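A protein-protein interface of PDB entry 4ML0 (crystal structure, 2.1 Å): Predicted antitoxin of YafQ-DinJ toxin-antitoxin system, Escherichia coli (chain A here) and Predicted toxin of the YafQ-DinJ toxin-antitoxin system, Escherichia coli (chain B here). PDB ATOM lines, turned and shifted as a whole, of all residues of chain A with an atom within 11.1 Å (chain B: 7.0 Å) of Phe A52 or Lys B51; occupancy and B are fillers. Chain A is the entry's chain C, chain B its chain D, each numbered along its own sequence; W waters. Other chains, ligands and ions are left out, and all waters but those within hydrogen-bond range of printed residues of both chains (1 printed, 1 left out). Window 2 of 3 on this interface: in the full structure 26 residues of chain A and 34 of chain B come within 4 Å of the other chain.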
ATOM      1  N   THR A  40     -11.501   5.115  23.823  1.00  0.00           N
ATOM      2  CA  THR A  40     -10.926   3.805  24.121  1.00  0.00           C
ATOM      3  C   THR A  40     -11.527   2.697  23.240  1.00  0.00           C
ATOM      4  O   THR A  40     -10.802   1.842  22.728  1.00  0.00           O
ATOM      5  CB  THR A  40     -11.118   3.447  25.608  1.00  0.00           C
ATOM      6  OG1 THR A  40     -10.532   4.476  26.405  1.00  0.00           O
ATOM      7  CG2 THR A  40     -10.429   2.135  25.946  1.00  0.00           C
ATOM      8  N   LYS A  43     -10.074   2.949  19.769  1.00  0.00           N
ATOM      9  CA  LYS A  43      -8.735   2.369  19.672  1.00  0.00           C
ATOM     10  C   LYS A  43      -8.800   0.835  19.660  1.00  0.00           C
ATOM     11  O   LYS A  43      -8.153   0.187  18.830  1.00  0.00           O
ATOM     12  CB  LYS A  43      -7.841   2.855  20.818  1.00  0.00           C
ATOM     13  CG  LYS A  43      -6.402   2.335  20.737  1.00  0.00           C
ATOM     14  CD  LYS A  43      -5.554   2.823  21.923  1.00  0.00           C
ATOM     15  CE  LYS A  43      -4.150   2.185  21.903  1.00  0.00           C
ATOM     16  NZ  LYS A  43      -3.314   2.676  20.772  1.00  0.00           N
ATOM     17  N   VAL A  44      -9.589   0.257  20.567  1.00  0.00           N
ATOM     18  CA  VAL A  44      -9.778  -1.199  20.575  1.00  0.00           C
ATOM     19  C   VAL A  44     -10.305  -1.745  19.234  1.00  0.00           C
ATOM     20  O   VAL A  44      -9.774  -2.729  18.709  1.00  0.00           O
ATOM     21  CB  VAL A  44     -10.705  -1.637  21.749  1.00  0.00           C
ATOM     22  CG1 VAL A  44     -11.177  -3.071  21.561  1.00  0.00           C
ATOM     23  CG2 VAL A  44      -9.968  -1.479  23.077  1.00  0.00           C
ATOM     24  N   ARG A  46     -10.193  -0.335  16.187  1.00  0.00           N
ATOM     25  CA  ARG A  46      -9.252  -0.170  15.076  1.00  0.00           C
ATOM     26  C   ARG A  46      -8.080  -1.123  15.168  1.00  0.00           C
ATOM     27  O   ARG A  46      -7.642  -1.670  14.157  1.00  0.00           O
ATOM     28  CB  ARG A  46      -8.710   1.257  15.016  1.00  0.00           C
ATOM     29  CG  ARG A  46      -9.735   2.237  14.554  1.00  0.00           C
ATOM     30  CD  ARG A  46      -9.170   3.637  14.493  1.00  0.00           C
ATOM     31  NE  ARG A  46     -10.205   4.623  14.145  1.00  0.00           N
ATOM     32  CZ  ARG A  46     -10.142   5.898  14.508  1.00  0.00           C
ATOM     33  NH1 ARG A  46      -9.105   6.319  15.245  1.00  0.00           N
ATOM     34  NH2 ARG A  46     -11.118   6.735  14.164  1.00  0.00           N
ATOM     35  N   GLU A  47      -7.547  -1.304  16.373  1.00  0.00           N
ATOM     36  CA  GLU A  47      -6.308  -2.059  16.506  1.00  0.00           C
ATOM     37  C   GLU A  47      -6.549  -3.536  16.721  1.00  0.00           C
ATOM     38  O   GLU A  47      -5.633  -4.337  16.571  1.00  0.00           O
ATOM     39  CB  GLU A  47      -5.436  -1.486  17.630  1.00  0.00           C
ATOM     40  CG  GLU A  47      -5.026  -0.051  17.357  1.00  0.00           C
ATOM     41  CD  GLU A  47      -4.189   0.558  18.485  1.00  0.00           C
ATOM     42  OE1 GLU A  47      -3.889  -0.159  19.468  1.00  0.00           O
ATOM     43  OE2 GLU A  47      -3.842   1.758  18.388  1.00  0.00           O
ATOM     44  N   LYS A  48      -7.787  -3.896  17.051  1.00  0.00           N
ATOM     45  CA  LYS A  48      -8.115  -5.283  17.403  1.00  0.00           C
ATOM     46  C   LYS A  48      -7.177  -5.737  18.519  1.00  0.00           C
ATOM     47  O   LYS A  48      -6.676  -6.861  18.508  1.00  0.00           O
ATOM     48  CB  LYS A  48      -7.984  -6.229  16.195  1.00  0.00           C
ATOM     49  CG  LYS A  48      -8.334  -5.585  14.851  1.00  0.00           C
ATOM     50  CD  LYS A  48      -9.810  -5.350  14.716  1.00  0.00           C
ATOM     51  CE  LYS A  48     -10.181  -4.955  13.268  1.00  0.00           C
ATOM     52  NZ  LYS A  48      -9.703  -3.598  12.864  1.00  0.00           N
ATOM     53  N   ALA A  49      -6.932  -4.845  19.475  1.00  0.00           N
ATOM     54  CA  ALA A  49      -6.050  -5.141  20.591  1.00  0.00           C
ATOM     55  C   ALA A  49      -6.396  -4.226  21.763  1.00  0.00           C
ATOM     56  O   ALA A  49      -7.118  -3.241  21.600  1.00  0.00           O
ATOM     57  CB  ALA A  49      -4.600  -4.957  20.180  1.00  0.00           C
ATOM     58  N   LEU A  50      -5.865  -4.544  22.934  1.00  0.00           N
ATOM     59  CA  LEU A  50      -6.086  -3.725  24.115  1.00  0.00           C
ATOM     60  C   LEU A  50      -5.024  -2.640  24.183  1.00  0.00           C
ATOM     61  O   LEU A  50      -3.898  -2.854  23.741  1.00  0.00           O
ATOM     62  CB  LEU A  50      -5.966  -4.597  25.367  1.00  0.00           C
ATOM     63  CG  LEU A  50      -7.216  -4.976  26.146  1.00  0.00           C
ATOM     64  CD1 LEU A  50      -8.288  -5.468  25.210  1.00  0.00           C
ATOM     65  CD2 LEU A  50      -6.882  -6.043  27.189  1.00  0.00           C
ATOM     66  N   PRO A  51      -5.365  -1.472  24.752  1.00  0.00           N
ATOM     67  CA  PRO A  51      -4.331  -0.485  25.108  1.00  0.00           C
ATOM     68  C   PRO A  51      -3.330  -1.117  26.093  1.00  0.00           C
ATOM     69  O   PRO A  51      -3.703  -2.099  26.753  1.00  0.00           O
ATOM     70  CB  PRO A  51      -5.125   0.611  25.826  1.00  0.00           C
ATOM     71  CG  PRO A  51      -6.551   0.460  25.311  1.00  0.00           C
ATOM     72  CD  PRO A  51      -6.727  -1.023  25.098  1.00  0.00           C
ATOM     73  N   PHE A  52      -2.109  -0.575  26.198  1.00  0.00           N
ATOM     74  CA  PHE A  52      -1.057  -1.172  27.045  1.00  0.00           C
ATOM     75  C   PHE A  52      -1.335  -0.969  28.522  1.00  0.00           C
ATOM     76  O   PHE A  52      -2.007  -0.013  28.900  1.00  0.00           O
ATOM     77  CB  PHE A  52       0.318  -0.533  26.775  1.00  0.00           C
ATOM     78  CG  PHE A  52       0.900  -0.832  25.412  1.00  0.00           C
ATOM     79  CD1 PHE A  52       0.456  -1.909  24.658  1.00  0.00           C
ATOM     80  CD2 PHE A  52       1.914  -0.021  24.895  1.00  0.00           C
ATOM     81  CE1 PHE A  52       1.008  -2.173  23.394  1.00  0.00           C
ATOM     82  CE2 PHE A  52       2.478  -0.281  23.647  1.00  0.00           C
ATOM     83  CZ  PHE A  52       2.023  -1.352  22.892  1.00  0.00           C
ATOM     84  N   ASP A  53      -0.781  -1.847  29.356  1.00  0.00           N
ATOM     85  CA  ASP A  53      -0.690  -1.606  30.804  1.00  0.00           C
ATOM     86  C   ASP A  53      -2.022  -1.285  31.482  1.00  0.00           C
ATOM     87  O   ASP A  53      -2.054  -0.494  32.427  1.00  0.00           O
ATOM     88  CB  ASP A  53       0.273  -0.441  31.109  1.00  0.00           C
ATOM     89  CG  ASP A  53       1.637  -0.583  30.430  1.00  0.00           C
ATOM     90  OD1 ASP A  53       2.053  -1.715  30.123  1.00  0.00           O
ATOM     91  OD2 ASP A  53       2.296   0.460  30.207  1.00  0.00           O
ATOM     92  N   LEU A  54      -3.119  -1.864  31.007  1.00  0.00           N
ATOM     93  CA  LEU A  54      -4.408  -1.575  31.643  1.00  0.00           C
ATOM     94  C   LEU A  54      -4.479  -2.171  33.052  1.00  0.00           C
ATOM     95  O   LEU A  54      -5.126  -1.610  33.945  1.00  0.00           O
ATOM     96  CB  LEU A  54      -5.576  -2.070  30.793  1.00  0.00           C
ATOM     97  CG  LEU A  54      -5.937  -1.258  29.545  1.00  0.00           C
ATOM     98  CD1 LEU A  54      -7.071  -1.931  28.846  1.00  0.00           C
ATOM     99  CD2 LEU A  54      -6.331   0.177  29.873  1.00  0.00           C
ATOM    100  N   ARG A  55      -3.802  -3.303  33.250  1.00  0.00           N
ATOM    101  CA  ARG A  55      -3.803  -4.000  34.544  1.00  0.00           C
ATOM    102  C   ARG A  55      -2.378  -4.342  34.972  1.00  0.00           C
ATOM    103  O   ARG A  55      -1.539  -4.689  34.138  1.00  0.00           O
ATOM    104  CB  ARG A  55      -4.667  -5.278  34.471  1.00  0.00           C
ATOM    105  CG  ARG A  55      -6.165  -5.028  34.294  1.00  0.00           C
ATOM    106  CD  ARG A  55      -6.968  -6.298  33.943  1.00  0.00           C
ATOM    107  NE  ARG A  55      -6.715  -6.784  32.577  1.00  0.00           N
ATOM    108  CZ  ARG A  55      -7.238  -7.899  32.063  1.00  0.00           C
ATOM    109  NH1 ARG A  55      -8.059  -8.652  32.794  1.00  0.00           N
ATOM    110  NH2 ARG A  55      -6.952  -8.258  30.817  1.00  0.00           N
ATOM    111  N   GLU A  56      -2.110  -4.237  36.270  1.00  0.00           N
ATOM    112  CA  GLU A  56      -0.795  -4.580  36.811  1.00  0.00           C
ATOM    113  C   GLU A  56      -0.603  -6.099  36.779  1.00  0.00           C
ATOM    114  O   GLU A  56      -1.589  -6.846  36.742  1.00  0.00           O
ATOM    115  CB  GLU A  56      -0.685  -4.063  38.249  1.00  0.00           C
ATOM    116  CG  GLU A  56      -0.631  -2.541  38.357  1.00  0.00           C
ATOM    117  CD  GLU A  56      -0.989  -2.033  39.751  1.00  0.00           C
ATOM    118  OE1 GLU A  56      -1.850  -2.655  40.415  1.00  0.00           O
ATOM    119  OE2 GLU A  56      -0.413  -1.011  40.183  1.00  0.00           O
ATOM    120  N   PRO A  57       0.661  -6.567  36.790  1.00  0.00           N
ATOM    121  CA  PRO A  57       0.868  -8.024  36.747  1.00  0.00           C
ATOM    122  C   PRO A  57       0.130  -8.700  37.911  1.00  0.00           C
ATOM    123  O   PRO A  57       0.076  -8.142  39.016  1.00  0.00           O
ATOM    124  CB  PRO A  57       2.381  -8.168  36.929  1.00  0.00           C
ATOM    125  CG  PRO A  57       2.957  -6.846  36.458  1.00  0.00           C
ATOM    126  CD  PRO A  57       1.934  -5.821  36.880  1.00  0.00           C
ATOM    127  N   LEU B  46      12.529  -4.789  18.034  1.00  0.00           N
ATOM    128  CA  LEU B  46      11.737  -5.793  17.336  1.00  0.00           C
ATOM    129  C   LEU B  46      10.834  -5.201  16.251  1.00  0.00           C
ATOM    130  O   LEU B  46      10.527  -4.004  16.274  1.00  0.00           O
ATOM    131  CB  LEU B  46      10.897  -6.553  18.371  1.00  0.00           C
ATOM    132  CG  LEU B  46      11.684  -7.199  19.521  1.00  0.00           C
ATOM    133  CD1 LEU B  46      10.812  -7.437  20.756  1.00  0.00           C
ATOM    134  CD2 LEU B  46      12.290  -8.514  19.061  1.00  0.00           C
ATOM    135  N   PRO B  47      10.411  -6.042  15.289  1.00  0.00           N
ATOM    136  CA  PRO B  47       9.305  -5.701  14.386  1.00  0.00           C
ATOM    137  C   PRO B  47       8.157  -5.072  15.180  1.00  0.00           C
ATOM    138  O   PRO B  47       7.932  -5.425  16.345  1.00  0.00           O
ATOM    139  CB  PRO B  47       8.876  -7.064  13.845  1.00  0.00           C
ATOM    140  CG  PRO B  47      10.170  -7.857  13.802  1.00  0.00           C
ATOM    141  CD  PRO B  47      11.008  -7.354  14.967  1.00  0.00           C
ATOM    142  N   ALA B  48       7.443  -4.145  14.556  1.00  0.00           N
ATOM    143  CA  ALA B  48       6.452  -3.348  15.272  1.00  0.00           C
ATOM    144  C   ALA B  48       5.261  -4.169  15.742  1.00  0.00           C
ATOM    145  O   ALA B  48       4.594  -3.791  16.713  1.00  0.00           O
ATOM    146  CB  ALA B  48       5.994  -2.169  14.414  1.00  0.00           C
ATOM    147  N   VAL B  49       4.992  -5.282  15.052  1.00  0.00           N
ATOM    148  CA  VAL B  49       3.838  -6.127  15.372  1.00  0.00           C
ATOM    149  C   VAL B  49       3.900  -6.661  16.794  1.00  0.00           C
ATOM    150  O   VAL B  49       2.871  -6.991  17.386  1.00  0.00           O
ATOM    151  CB  VAL B  49       3.728  -7.351  14.445  1.00  0.00           C
ATOM    152  CG1 VAL B  49       2.934  -7.025  13.195  1.00  0.00           C
ATOM    153  CG2 VAL B  49       5.123  -7.893  14.112  1.00  0.00           C
ATOM    154  N   TYR B  50       5.110  -6.763  17.332  1.00  0.00           N
ATOM    155  CA  TYR B  50       5.290  -7.309  18.671  1.00  0.00           C
ATOM    156  C   TYR B  50       4.869  -6.339  19.768  1.00  0.00           C
ATOM    157  O   TYR B  50       4.739  -6.739  20.931  1.00  0.00           O
ATOM    158  CB  TYR B  50       6.734  -7.784  18.878  1.00  0.00           C
ATOM    159  CG  TYR B  50       7.059  -8.976  18.016  1.00  0.00           C
ATOM    160  CD1 TYR B  50       6.333 -10.156  18.142  1.00  0.00           C
ATOM    161  CD2 TYR B  50       8.077  -8.928  17.072  1.00  0.00           C
ATOM    162  CE1 TYR B  50       6.607 -11.249  17.364  1.00  0.00           C
ATOM    163  CE2 TYR B  50       8.364 -10.030  16.285  1.00  0.00           C
ATOM    164  CZ  TYR B  50       7.624 -11.184  16.438  1.00  0.00           C
ATOM    165  OH  TYR B  50       7.884 -12.289  15.661  1.00  0.00           O
ATOM    166  N   LYS B  51       4.665  -5.071  19.407  1.00  0.00           N
ATOM    167  CA  LYS B  51       4.181  -4.062  20.362  1.00  0.00           C
ATOM    168  C   LYS B  51       5.016  -4.053  21.644  1.00  0.00           C
ATOM    169  O   LYS B  51       4.474  -3.903  22.747  1.00  0.00           O
ATOM    170  CB  LYS B  51       2.707  -4.323  20.725  1.00  0.00           C
ATOM    171  CG  LYS B  51       1.748  -4.383  19.514  1.00  0.00           C
ATOM    172  CD  LYS B  51       1.749  -3.065  18.748  1.00  0.00           C
ATOM    173  CE  LYS B  51       0.889  -3.156  17.482  1.00  0.00           C
ATOM    174  NZ  LYS B  51       0.961  -1.907  16.659  1.00  0.00           N
ATOM    175  N   ASP B  52       6.326  -4.220  21.499  1.00  0.00           N
ATOM    176  CA  ASP B  52       7.217  -4.346  22.651  1.00  0.00           C
ATOM    177  C   ASP B  52       7.211  -3.088  23.528  1.00  0.00           C
ATOM    178  O   ASP B  52       7.292  -1.963  23.024  1.00  0.00           O
ATOM    179  CB  ASP B  52       8.641  -4.661  22.185  1.00  0.00           C
ATOM    180  CG  ASP B  52       9.564  -5.013  23.336  1.00  0.00           C
ATOM    181  OD1 ASP B  52       9.301  -6.032  24.009  1.00  0.00           O
ATOM    182  OD2 ASP B  52      10.552  -4.286  23.571  1.00  0.00           O
ATOM    183  N   HIS B  53       7.103  -3.268  24.843  1.00  0.00           N
ATOM    184  CA  HIS B  53       7.107  -2.122  25.748  1.00  0.00           C
ATOM    185  C   HIS B  53       7.515  -2.553  27.150  1.00  0.00           C
ATOM    186  O   HIS B  53       7.416  -3.742  27.469  1.00  0.00           O
ATOM    187  CB  HIS B  53       5.717  -1.474  25.764  1.00  0.00           C
ATOM    188  CG  HIS B  53       4.627  -2.403  26.191  1.00  0.00           C
ATOM    189  ND1 HIS B  53       4.119  -3.382  25.361  1.00  0.00           N
ATOM    190  CD2 HIS B  53       3.939  -2.501  27.354  1.00  0.00           C
ATOM    191  CE1 HIS B  53       3.164  -4.042  25.995  1.00  0.00           C
ATOM    192  NE2 HIS B  53       3.032  -3.527  27.205  1.00  0.00           N
ATOM    193  N   PRO B  54       7.979  -1.595  27.986  1.00  0.00           N
ATOM    194  CA  PRO B  54       8.337  -1.939  29.371  1.00  0.00           C
ATOM    195  C   PRO B  54       7.132  -2.453  30.165  1.00  0.00           C
ATOM    196  O   PRO B  54       6.012  -1.955  30.000  1.00  0.00           O
ATOM    197  CB  PRO B  54       8.780  -0.593  29.979  1.00  0.00           C
ATOM    198  CG  PRO B  54       9.098   0.302  28.798  1.00  0.00           C
ATOM    199  CD  PRO B  54       8.180  -0.159  27.691  1.00  0.00           C
ATOM    200  N   GLN B  56       4.901  -2.546  33.337  1.00  0.00           N
ATOM    201  CA  GLN B  56       4.629  -1.633  34.444  1.00  0.00           C
ATOM    202  C   GLN B  56       4.675  -2.344  35.803  1.00  0.00           C
ATOM    203  O   GLN B  56       3.714  -3.010  36.212  1.00  0.00           O
ATOM    204  CB  GLN B  56       3.307  -0.883  34.240  1.00  0.00           C
ATOM    205  CG  GLN B  56       3.424   0.243  33.201  1.00  0.00           C
ATOM    206  CD  GLN B  56       2.448   1.408  33.435  1.00  0.00           C
ATOM    207  OE1 GLN B  56       1.398   1.251  34.087  1.00  0.00           O
ATOM    208  NE2 GLN B  56       2.799   2.588  32.897  1.00  0.00           N
ATOM    209  N   ARG B  63      10.112  -6.404  30.417  1.00  0.00           N
ATOM    210  CA  ARG B  63       9.406  -5.953  29.231  1.00  0.00           C
ATOM    211  C   ARG B  63       8.346  -6.963  28.824  1.00  0.00           C
ATOM    212  O   ARG B  63       8.326  -8.103  29.299  1.00  0.00           O
ATOM    213  CB  ARG B  63      10.385  -5.710  28.078  1.00  0.00           C
ATOM    214  CG  ARG B  63      11.384  -4.590  28.337  1.00  0.00           C
ATOM    215  CD  ARG B  63      12.296  -4.363  27.127  1.00  0.00           C
ATOM    216  NE  ARG B  63      11.609  -3.741  25.993  1.00  0.00           N
ATOM    217  CZ  ARG B  63      11.312  -2.444  25.913  1.00  0.00           C
ATOM    218  NH1 ARG B  63      11.630  -1.628  26.913  1.00  0.00           N
ATOM    219  NH2 ARG B  63      10.697  -1.961  24.833  1.00  0.00           N
ATOM    220  N   ASP B  64       7.495  -6.536  27.911  1.00  0.00           N
ATOM    221  CA  ASP B  64       6.261  -7.220  27.588  1.00  0.00           C
ATOM    222  C   ASP B  64       6.143  -7.106  26.066  1.00  0.00           C
ATOM    223  O   ASP B  64       6.067  -5.994  25.542  1.00  0.00           O
ATOM    224  CB  ASP B  64       5.146  -6.439  28.309  1.00  0.00           C
ATOM    225  CG  ASP B  64       3.742  -6.861  27.924  1.00  0.00           C
ATOM    226  OD1 ASP B  64       3.497  -7.276  26.773  1.00  0.00           O
ATOM    227  OD2 ASP B  64       2.848  -6.721  28.792  1.00  0.00           O
ATOM    228  N   ALA B  65       6.150  -8.240  25.361  1.00  0.00           N
ATOM    229  CA  ALA B  65       5.987  -8.260  23.904  1.00  0.00           C
ATOM    230  C   ALA B  65       4.800  -9.145  23.541  1.00  0.00           C
ATOM    231  O   ALA B  65       4.523 -10.127  24.233  1.00  0.00           O
ATOM    232  CB  ALA B  65       7.257  -8.774  23.230  1.00  0.00           C
ATOM    233  N   HIS B  66       4.119  -8.823  22.444  1.00  0.00           N
ATOM    234  CA  HIS B  66       2.916  -9.559  22.069  1.00  0.00           C
ATOM    235  C   HIS B  66       3.173 -10.517  20.909  1.00  0.00           C
ATOM    236  O   HIS B  66       3.411 -10.089  19.776  1.00  0.00           O
ATOM    237  CB  HIS B  66       1.757  -8.595  21.747  1.00  0.00           C
ATOM    238  CG  HIS B  66       1.276  -7.813  22.934  1.00  0.00           C
ATOM    239  ND1 HIS B  66       0.171  -6.989  22.888  1.00  0.00           N
ATOM    240  CD2 HIS B  66       1.754  -7.729  24.202  1.00  0.00           C
ATOM    241  CE1 HIS B  66      -0.014  -6.435  24.075  1.00  0.00           C
ATOM    242  NE2 HIS B  66       0.930  -6.867  24.891  1.00  0.00           N
ATOM    243  N   HIS B  90      -3.630 -12.140  28.393  1.00  0.00           N
ATOM    244  CA  HIS B  90      -3.765 -11.000  29.300  1.00  0.00           C
ATOM    245  C   HIS B  90      -4.341 -11.462  30.626  1.00  0.00           C
ATOM    246  O   HIS B  90      -3.854 -11.080  31.688  1.00  0.00           O
ATOM    247  CB  HIS B  90      -4.697  -9.927  28.727  1.00  0.00           C
ATOM    248  CG  HIS B  90      -4.037  -9.005  27.757  1.00  0.00           C
ATOM    249  ND1 HIS B  90      -4.158  -9.150  26.392  1.00  0.00           N
ATOM    250  CD2 HIS B  90      -3.249  -7.918  27.955  1.00  0.00           C
ATOM    251  CE1 HIS B  90      -3.478  -8.188  25.789  1.00  0.00           C
ATOM    252  NE2 HIS B  90      -2.911  -7.434  26.713  1.00  0.00           N
HETATM  253  O   HOH W   1       4.838   0.491  29.492  1.00  0.00           O
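The backbone carbonyl oxygen (O) of Lys B51 sits at hydrogen-bond distance from a ring nitrogen (ND1) of His B53, 2.7 Å away. The backbone carbonyl oxygen (O) of His B53 lies within hydrogen-bond range of the backbone NH (N) of Asp B64, 2.8 Å away.
Water W1 bridges the side-chain carboxylate of Asp A53 (2.6 Å) and the backbone carbonyl oxygen of Pro B54 (2.8 Å).
Hydrophobic or aromatic side chains of chain B that line the printed part of chain A: His B53 and His B90. Of the 15 printed residues of chain A, 4 touch a printed residue of chain B. Hydrophobic or aromatic side chains of chain A within 4 Å of the printed part of chain B: Phe A52 and Pro A57. Among the printed residues, 7 pairs touch across the chains. Among the printed residues, no Asp or Glu carboxylate lies within 4 Å of a Lys or Arg side-chain nitrogen of the other chain.
Among the printed residues, pairs that only touch across the chains: Pro A57 with Gln B56, Asp A53 with His B53, Arg A55 with His B90, Phe A52 with Lys B51, Phe A52 with His B53 and Asp A53 with Pro B54.
Printed residues of chain B within 4 Å of Arg A55: His B90 (3.5 Å). Printed residues of chain B within 4 Å of Pro A57: Gln B56. No residue of chain A comes within 4 Å of Ala B48. No residue of chain A comes within 4 Å of Val B49. Lys B51 touches just one residue of chain A: Phe A52. Of chain A, only Phe A52 (3.7 Å) and Asp A53 (3.4 Å) come within 4 Å of His B53. Printed residues of chain A within 4 Å of Pro B54: Asp A53 (3.97 Å). No residue of chain A comes within 4 Å of Ala B65. No residue of chain A comes within 4 Å of His B66. Of the printed residues of chain A, His B90 touches Arg A55 (3.5 Å). The nearest residue of chain B that does not touch Phe A52 is His B66 (4.4 Å). The nearest residue of chain A that does not touch Lys B51 is Glu A47 (5.9 Å).
The side-chain amide nitrogen (NE2) of Gln B56 lies close to the side-chain carboxylate (OD2) of Asp A53 (3.5 Å).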
